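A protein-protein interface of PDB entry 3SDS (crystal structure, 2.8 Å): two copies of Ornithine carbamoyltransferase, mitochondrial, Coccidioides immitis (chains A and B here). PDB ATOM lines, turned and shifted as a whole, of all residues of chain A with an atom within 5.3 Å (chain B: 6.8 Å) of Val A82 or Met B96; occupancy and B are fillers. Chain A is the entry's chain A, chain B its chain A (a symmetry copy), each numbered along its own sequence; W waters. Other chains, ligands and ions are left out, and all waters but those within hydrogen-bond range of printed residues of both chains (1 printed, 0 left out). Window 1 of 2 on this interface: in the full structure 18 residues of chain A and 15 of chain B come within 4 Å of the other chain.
The backbone carbonyl oxygen (O) of Phe B97 is in hydrogen-bond range of the guanidinium group (NH2) of Arg A81 (3.0 Å).
The side-chain carboxylate of Glu A85 is in hydrogen-bond range of a ring nitrogen (NE2) of His B94 (3.1 Å).
The backbone carbonyl oxygen (O) of Thr A80 sits at hydrogen-bond distance from the side-chain hydroxyl (OG) of Ser A83, at 3.1 Å.
The guanidinium group (NE) of Arg A81 is in salt-bridge range of the side-chain carboxylate (OE1) of Glu A85.
N of Val B69 lies within hydrogen-bond range of O of His B94, at 2.8 Å.
O of Val B69 sits at hydrogen-bond distance from N of Met B96, at 2.8 Å.
N of Met B71 sits at hydrogen-bond distance from O of Met B96.
The backbone NH (N) of Leu B98 sits at hydrogen-bond distance from the backbone carbonyl oxygen (O) of Met B71.
Among the printed residues, merely in contact across the chains: Arg A79 with Val B117, Arg A81 with Leu B98, Val A82 with Met B96, Ser A83 with Met B121, Glu A85 with Met B96 and Gly A86 with Thr B68.
Val A82 touches one residue of chain B.
Printed residues of chain A within 4 Å of Val B117: Arg A79 (3.7 Å).
Of the printed residues of chain A, Thr B68 touches Gly A86.
Of the printed residues of chain B, Gly A86 touches Thr B68 (3.9 Å).
Of the printed residues of chain B, Ser A83 touches Met B121.
Of the printed residues of chain B, Arg A81 touches Phe B97 and Leu B98.
Thr A84 touches none of the printed residues of chain B.
Ala A87 touches none of the printed residues of chain B.
The nearest residue of chain A that does not touch Met B96 is Arg A81 (4.4 Å).
The nearest printed residue of chain A that does not touch His B94 is Gly A86 (6.2 Å).
Printed residues of chain B that touch a printed residue of chain A: Thr B68, His B94, Met B96, Phe B97, Leu B98, Val B117 and Met B121.
Of the 10 printed residues of chain A, 6 touch a printed residue of chain B.
Among the printed residues, 8 pairs touch across the chains.
Among the printed residues, no Asp or Glu carboxylate lies within 4 Å of a Lys or Arg side-chain nitrogen of the other chain.
Position printed for both chains: 85.
Water W1 bridges the backbone carbonyl oxygen of Gly A86 (2.9 Å) and the side-chain hydroxyl of Thr B68 (2.9 Å).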
ATOM      1  N   THR A  78     -21.949   1.241  12.311  1.00  0.00           N
ATOM      2  CA  THR A  78     -23.112   0.851  11.540  1.00  0.00           C
ATOM      3  C   THR A  78     -23.427   1.754  10.345  1.00  0.00           C
ATOM      4  O   THR A  78     -23.668   1.253   9.235  1.00  0.00           O
ATOM      5  CB  THR A  78     -24.316   0.725  12.460  1.00  0.00           C
ATOM      6  OG1 THR A  78     -24.126  -0.429  13.291  1.00  0.00           O
ATOM      7  CG2 THR A  78     -25.591   0.531  11.655  1.00  0.00           C
ATOM      8  N   ARG A  79     -23.418   3.066  10.568  1.00  0.00           N
ATOM      9  CA  ARG A  79     -23.669   4.011   9.498  1.00  0.00           C
ATOM     10  C   ARG A  79     -22.748   3.759   8.295  1.00  0.00           C
ATOM     11  O   ARG A  79     -23.235   3.649   7.155  1.00  0.00           O
ATOM     12  CB  ARG A  79     -23.559   5.457   9.998  1.00  0.00           C
ATOM     13  CG  ARG A  79     -24.064   6.509   8.987  1.00  0.00           C
ATOM     14  CD  ARG A  79     -25.100   7.448   9.623  1.00  0.00           C
ATOM     15  NE  ARG A  79     -26.257   6.687  10.120  1.00  0.00           N
ATOM     16  CZ  ARG A  79     -27.189   7.162  10.951  1.00  0.00           C
ATOM     17  NH1 ARG A  79     -28.186   6.380  11.351  1.00  0.00           N
ATOM     18  NH2 ARG A  79     -27.130   8.412  11.393  1.00  0.00           N
ATOM     19  N   THR A  80     -21.434   3.659   8.538  1.00  0.00           N
ATOM     20  CA  THR A  80     -20.479   3.374   7.449  1.00  0.00           C
ATOM     21  C   THR A  80     -20.776   2.040   6.744  1.00  0.00           C
ATOM     22  O   THR A  80     -20.678   1.950   5.491  1.00  0.00           O
ATOM     23  CB  THR A  80     -18.985   3.462   7.896  1.00  0.00           C
ATOM     24  OG1 THR A  80     -18.545   4.821   7.785  1.00  0.00           O
ATOM     25  CG2 THR A  80     -18.056   2.567   7.016  1.00  0.00           C
ATOM     26  N   ARG A  81     -21.169   1.044   7.495  1.00  0.00           N
ATOM     27  CA  ARG A  81     -21.493  -0.237   6.948  1.00  0.00           C
ATOM     28  C   ARG A  81     -22.634  -0.147   5.988  1.00  0.00           C
ATOM     29  O   ARG A  81     -22.602  -0.691   4.941  1.00  0.00           O
ATOM     30  CB  ARG A  81     -21.926  -1.119   8.080  1.00  0.00           C
ATOM     31  CG  ARG A  81     -21.245  -2.409   8.133  1.00  0.00           C
ATOM     32  CD  ARG A  81     -21.904  -3.289   9.100  1.00  0.00           C
ATOM     33  NE  ARG A  81     -22.578  -4.356   8.413  1.00  0.00           N
ATOM     34  CZ  ARG A  81     -23.299  -5.261   9.019  1.00  0.00           C
ATOM     35  NH1 ARG A  81     -23.446  -5.216  10.307  1.00  0.00           N
ATOM     36  NH2 ARG A  81     -23.863  -6.198   8.332  1.00  0.00           N
ATOM     37  N   VAL A  82     -23.681   0.529   6.384  1.00  0.00           N
ATOM     38  CA  VAL A  82     -24.895   0.620   5.575  1.00  0.00           C
ATOM     39  C   VAL A  82     -24.625   1.109   4.150  1.00  0.00           C
ATOM     40  O   VAL A  82     -25.116   0.515   3.204  1.00  0.00           O
ATOM     41  CB  VAL A  82     -25.998   1.472   6.239  1.00  0.00           C
ATOM     42  CG1 VAL A  82     -27.249   1.510   5.359  1.00  0.00           C
ATOM     43  CG2 VAL A  82     -26.329   0.941   7.628  1.00  0.00           C
ATOM     44  N   SER A  83     -23.843   2.174   4.002  1.00  0.00           N
ATOM     45  CA  SER A  83     -23.530   2.760   2.691  1.00  0.00           C
ATOM     46  C   SER A  83     -22.514   1.963   1.834  1.00  0.00           C
ATOM     47  O   SER A  83     -22.651   1.896   0.600  1.00  0.00           O
ATOM     48  CB  SER A  83     -23.041   4.193   2.870  1.00  0.00           C
ATOM     49  OG  SER A  83     -21.888   4.242   3.707  1.00  0.00           O
ATOM     50  N   THR A  84     -21.484   1.393   2.471  1.00  0.00           N
ATOM     51  CA  THR A  84     -20.510   0.551   1.755  1.00  0.00           C
ATOM     52  C   THR A  84     -21.251  -0.679   1.229  1.00  0.00           C
ATOM     53  O   THR A  84     -21.161  -1.044   0.042  1.00  0.00           O
ATOM     54  CB  THR A  84     -19.308   0.126   2.680  1.00  0.00           C
ATOM     55  OG1 THR A  84     -18.811   1.264   3.415  1.00  0.00           O
ATOM     56  CG2 THR A  84     -18.163  -0.485   1.883  1.00  0.00           C
ATOM     57  N   GLU A  85     -22.020  -1.298   2.112  1.00  0.00           N
ATOM     58  CA  GLU A  85     -22.753  -2.482   1.740  1.00  0.00           C
ATOM     59  C   GLU A  85     -23.604  -2.171   0.484  1.00  0.00           C
ATOM     60  O   GLU A  85     -23.443  -2.826  -0.561  1.00  0.00           O
ATOM     61  CB  GLU A  85     -23.542  -3.034   2.935  1.00  0.00           C
ATOM     62  CG  GLU A  85     -23.628  -4.558   2.920  1.00  0.00           C
ATOM     63  CD  GLU A  85     -23.658  -5.273   4.297  1.00  0.00           C
ATOM     64  OE1 GLU A  85     -23.027  -4.838   5.285  1.00  0.00           O
ATOM     65  OE2 GLU A  85     -24.305  -6.338   4.361  1.00  0.00           O
ATOM     66  N   GLY A  86     -24.437  -1.127   0.560  1.00  0.00           N
ATOM     67  CA  GLY A  86     -25.316  -0.731  -0.556  1.00  0.00           C
ATOM     68  C   GLY A  86     -24.591  -0.404  -1.851  1.00  0.00           C
ATOM     69  O   GLY A  86     -25.066  -0.740  -2.942  1.00  0.00           O
ATOM     70  N   ALA A  87     -23.436   0.246  -1.731  1.00  0.00           N
ATOM     71  CA  ALA A  87     -22.631   0.645  -2.882  1.00  0.00           C
ATOM     72  C   ALA A  87     -22.033  -0.533  -3.631  1.00  0.00           C
ATOM     73  O   ALA A  87     -22.105  -0.603  -4.864  1.00  0.00           O
ATOM     74  CB  ALA A  87     -21.540   1.584  -2.450  1.00  0.00           C
ATOM     75  N   THR B  68     -30.788  -3.712  -1.926  1.00  0.00           N
ATOM     76  CA  THR B  68     -30.536  -4.171  -0.554  1.00  0.00           C
ATOM     77  C   THR B  68     -31.812  -4.181   0.282  1.00  0.00           C
ATOM     78  O   THR B  68     -32.617  -3.229   0.216  1.00  0.00           O
ATOM     79  CB  THR B  68     -29.530  -3.252   0.136  1.00  0.00           C
ATOM     80  OG1 THR B  68     -28.362  -3.147  -0.683  1.00  0.00           O
ATOM     81  CG2 THR B  68     -29.151  -3.784   1.510  1.00  0.00           C
ATOM     82  N   VAL B  69     -31.993  -5.246   1.058  1.00  0.00           N
ATOM     83  CA  VAL B  69     -33.049  -5.282   2.071  1.00  0.00           C
ATOM     84  C   VAL B  69     -32.398  -5.271   3.460  1.00  0.00           C
ATOM     85  O   VAL B  69     -31.555  -6.125   3.762  1.00  0.00           O
ATOM     86  CB  VAL B  69     -33.937  -6.531   1.897  1.00  0.00           C
ATOM     87  CG1 VAL B  69     -34.944  -6.673   3.054  1.00  0.00           C
ATOM     88  CG2 VAL B  69     -34.644  -6.495   0.566  1.00  0.00           C
ATOM     89  N   ALA B  70     -32.765  -4.315   4.308  1.00  0.00           N
ATOM     90  CA  ALA B  70     -32.198  -4.282   5.671  1.00  0.00           C
ATOM     91  C   ALA B  70     -33.018  -5.099   6.672  1.00  0.00           C
ATOM     92  O   ALA B  70     -34.241  -4.944   6.766  1.00  0.00           O
ATOM     93  CB  ALA B  70     -32.039  -2.849   6.160  1.00  0.00           C
ATOM     94  N   MET B  71     -32.347  -5.979   7.409  1.00  0.00           N
ATOM     95  CA  MET B  71     -32.984  -6.734   8.500  1.00  0.00           C
ATOM     96  C   MET B  71     -32.564  -6.151   9.849  1.00  0.00           C
ATOM     97  O   MET B  71     -31.378  -6.214  10.224  1.00  0.00           O
ATOM     98  CB  MET B  71     -32.600  -8.218   8.448  1.00  0.00           C
ATOM     99  CG  MET B  71     -32.811  -8.907   7.105  1.00  0.00           C
ATOM    100  SD  MET B  71     -32.270 -10.645   7.096  1.00  0.00           S
ATOM    101  CE  MET B  71     -30.491 -10.521   7.129  1.00  0.00           C
ATOM    102  N   MET B  72     -33.515  -5.565  10.571  1.00  0.00           N
ATOM    103  CA  MET B  72     -33.208  -4.991  11.900  1.00  0.00           C
ATOM    104  C   MET B  72     -33.764  -5.833  13.054  1.00  0.00           C
ATOM    105  O   MET B  72     -34.989  -5.887  13.264  1.00  0.00           O
ATOM    106  CB  MET B  72     -33.693  -3.546  12.009  1.00  0.00           C
ATOM    107  CG  MET B  72     -32.856  -2.576  11.207  1.00  0.00           C
ATOM    108  SD  MET B  72     -33.623  -0.956  11.008  1.00  0.00           S
ATOM    109  CE  MET B  72     -33.072  -0.141  12.507  1.00  0.00           C
ATOM    110  N   GLU B  85     -33.390 -14.263   4.628  1.00  0.00           N
ATOM    111  CA  GLU B  85     -32.164 -14.279   3.872  1.00  0.00           C
ATOM    112  C   GLU B  85     -32.392 -15.073   2.561  1.00  0.00           C
ATOM    113  O   GLU B  85     -32.213 -14.528   1.458  1.00  0.00           O
ATOM    114  CB  GLU B  85     -30.996 -14.778   4.734  1.00  0.00           C
ATOM    115  CG  GLU B  85     -29.678 -14.095   4.380  1.00  0.00           C
ATOM    116  CD  GLU B  85     -28.670 -13.871   5.539  1.00  0.00           C
ATOM    117  OE1 GLU B  85     -29.045 -13.617   6.705  1.00  0.00           O
ATOM    118  OE2 GLU B  85     -27.459 -13.906   5.242  1.00  0.00           O
ATOM    119  N   VAL B  88     -34.943 -13.299  -0.063  1.00  0.00           N
ATOM    120  CA  VAL B  88     -34.327 -12.193  -0.782  1.00  0.00           C
ATOM    121  C   VAL B  88     -33.416 -12.714  -1.902  1.00  0.00           C
ATOM    122  O   VAL B  88     -33.499 -12.242  -3.039  1.00  0.00           O
ATOM    123  CB  VAL B  88     -33.549 -11.285   0.191  1.00  0.00           C
ATOM    124  CG1 VAL B  88     -32.853 -10.136  -0.542  1.00  0.00           C
ATOM    125  CG2 VAL B  88     -34.488 -10.748   1.280  1.00  0.00           C
ATOM    126  N   HIS B  94     -29.767  -8.433  -2.222  1.00  0.00           N
ATOM    127  CA  HIS B  94     -28.873  -8.590  -1.060  1.00  0.00           C
ATOM    128  C   HIS B  94     -29.494  -8.280   0.329  1.00  0.00           C
ATOM    129  O   HIS B  94     -29.976  -7.170   0.576  1.00  0.00           O
ATOM    130  CB  HIS B  94     -27.583  -7.790  -1.252  1.00  0.00           C
ATOM    131  CG  HIS B  94     -26.650  -7.858  -0.076  1.00  0.00           C
ATOM    132  ND1 HIS B  94     -25.836  -8.947   0.171  1.00  0.00           N
ATOM    133  CD2 HIS B  94     -26.404  -6.973   0.922  1.00  0.00           C
ATOM    134  CE1 HIS B  94     -25.130  -8.727   1.269  1.00  0.00           C
ATOM    135  NE2 HIS B  94     -25.455  -7.536   1.745  1.00  0.00           N
ATOM    136  N   PRO B  95     -29.495  -9.272   1.230  1.00  0.00           N
ATOM    137  CA  PRO B  95     -29.953  -9.140   2.623  1.00  0.00           C
ATOM    138  C   PRO B  95     -28.882  -8.641   3.617  1.00  0.00           C
ATOM    139  O   PRO B  95     -27.797  -9.221   3.701  1.00  0.00           O
ATOM    140  CB  PRO B  95     -30.375 -10.567   2.973  1.00  0.00           C
ATOM    141  CG  PRO B  95     -29.533 -11.427   2.114  1.00  0.00           C
ATOM    142  CD  PRO B  95     -29.319 -10.686   0.845  1.00  0.00           C
ATOM    143  N   MET B  96     -29.188  -7.588   4.373  1.00  0.00           N
ATOM    144  CA  MET B  96     -28.188  -6.965   5.260  1.00  0.00           C
ATOM    145  C   MET B  96     -28.588  -7.133   6.727  1.00  0.00           C
ATOM    146  O   MET B  96     -29.651  -6.659   7.156  1.00  0.00           O
ATOM    147  CB  MET B  96     -27.982  -5.496   4.881  1.00  0.00           C
ATOM    148  CG  MET B  96     -27.183  -4.675   5.855  1.00  0.00           C
ATOM    149  SD  MET B  96     -26.872  -2.984   5.269  1.00  0.00           S
ATOM    150  CE  MET B  96     -28.480  -2.189   5.410  1.00  0.00           C
ATOM    151  N   PHE B  97     -27.745  -7.829   7.484  1.00  0.00           N
ATOM    152  CA  PHE B  97     -28.072  -8.172   8.871  1.00  0.00           C
ATOM    153  C   PHE B  97     -27.566  -7.123   9.842  1.00  0.00           C
ATOM    154  O   PHE B  97     -26.392  -6.844   9.899  1.00  0.00           O
ATOM    155  CB  PHE B  97     -27.519  -9.549   9.238  1.00  0.00           C
ATOM    156  CG  PHE B  97     -27.691  -9.900  10.686  1.00  0.00           C
ATOM    157  CD1 PHE B  97     -28.966 -10.001  11.252  1.00  0.00           C
ATOM    158  CD2 PHE B  97     -26.590 -10.151  11.490  1.00  0.00           C
ATOM    159  CE1 PHE B  97     -29.138 -10.337  12.621  1.00  0.00           C
ATOM    160  CE2 PHE B  97     -26.751 -10.498  12.856  1.00  0.00           C
ATOM    161  CZ  PHE B  97     -28.028 -10.589  13.419  1.00  0.00           C
ATOM    162  N   LEU B  98     -28.468  -6.509  10.579  1.00  0.00           N
ATOM    163  CA  LEU B  98     -28.064  -5.538  11.585  1.00  0.00           C
ATOM    164  C   LEU B  98     -28.707  -5.962  12.898  1.00  0.00           C
ATOM    165  O   LEU B  98     -29.910  -5.767  13.092  1.00  0.00           O
ATOM    166  CB  LEU B  98     -28.500  -4.120  11.189  1.00  0.00           C
ATOM    167  CG  LEU B  98     -28.230  -3.551   9.787  1.00  0.00           C
ATOM    168  CD1 LEU B  98     -29.046  -2.282   9.580  1.00  0.00           C
ATOM    169  CD2 LEU B  98     -26.759  -3.290   9.512  1.00  0.00           C
ATOM    170  N   VAL B 117     -32.660   8.061   7.704  1.00  0.00           N
ATOM    171  CA  VAL B 117     -31.327   7.744   7.157  1.00  0.00           C
ATOM    172  C   VAL B 117     -31.177   6.348   6.536  1.00  0.00           C
ATOM    173  O   VAL B 117     -30.726   6.223   5.396  1.00  0.00           O
ATOM    174  CB  VAL B 117     -30.217   7.982   8.223  1.00  0.00           C
ATOM    175  CG1 VAL B 117     -28.828   7.590   7.687  1.00  0.00           C
ATOM    176  CG2 VAL B 117     -30.214   9.439   8.645  1.00  0.00           C
ATOM    177  N   ILE B 118     -31.532   5.304   7.279  1.00  0.00           N
ATOM    178  CA  ILE B 118     -31.426   3.927   6.761  1.00  0.00           C
ATOM    179  C   ILE B 118     -32.345   3.714   5.570  1.00  0.00           C
ATOM    180  O   ILE B 118     -31.909   3.166   4.550  1.00  0.00           O
ATOM    181  CB  ILE B 118     -31.667   2.839   7.854  1.00  0.00           C
ATOM    182  CG1 ILE B 118     -30.587   2.955   8.938  1.00  0.00           C
ATOM    183  CG2 ILE B 118     -31.634   1.441   7.259  1.00  0.00           C
ATOM    184  CD1 ILE B 118     -30.533   1.802   9.941  1.00  0.00           C
ATOM    185  N   MET B 121     -31.250   4.658   1.922  1.00  0.00           N
ATOM    186  CA  MET B 121     -30.163   3.890   1.255  1.00  0.00           C
ATOM    187  C   MET B 121     -30.496   2.391   1.087  1.00  0.00           C
ATOM    188  O   MET B 121     -29.625   1.605   0.728  1.00  0.00           O
ATOM    189  CB  MET B 121     -28.785   4.086   1.950  1.00  0.00           C
ATOM    190  CG  MET B 121     -28.302   5.546   2.116  1.00  0.00           C
ATOM    191  SD  MET B 121     -26.661   5.771   2.924  1.00  0.00           S
ATOM    192  CE  MET B 121     -26.987   5.532   4.665  1.00  0.00           C
ATOM    193  N   VAL B 122     -31.749   1.999   1.334  1.00  0.00           N
ATOM    194  CA  VAL B 122     -32.203   0.616   1.076  1.00  0.00           C
ATOM    195  C   VAL B 122     -33.558   0.604   0.368  1.00  0.00           C
ATOM    196  O   VAL B 122     -34.225   1.654   0.266  1.00  0.00           O
ATOM    197  CB  VAL B 122     -32.279  -0.268   2.384  1.00  0.00           C
ATOM    198  CG1 VAL B 122     -30.983  -0.165   3.212  1.00  0.00           C
ATOM    199  CG2 VAL B 122     -33.483   0.083   3.232  1.00  0.00           C
HETATM  200  O   HOH W   1     -27.962  -1.105  -2.761  1.00  0.00           O
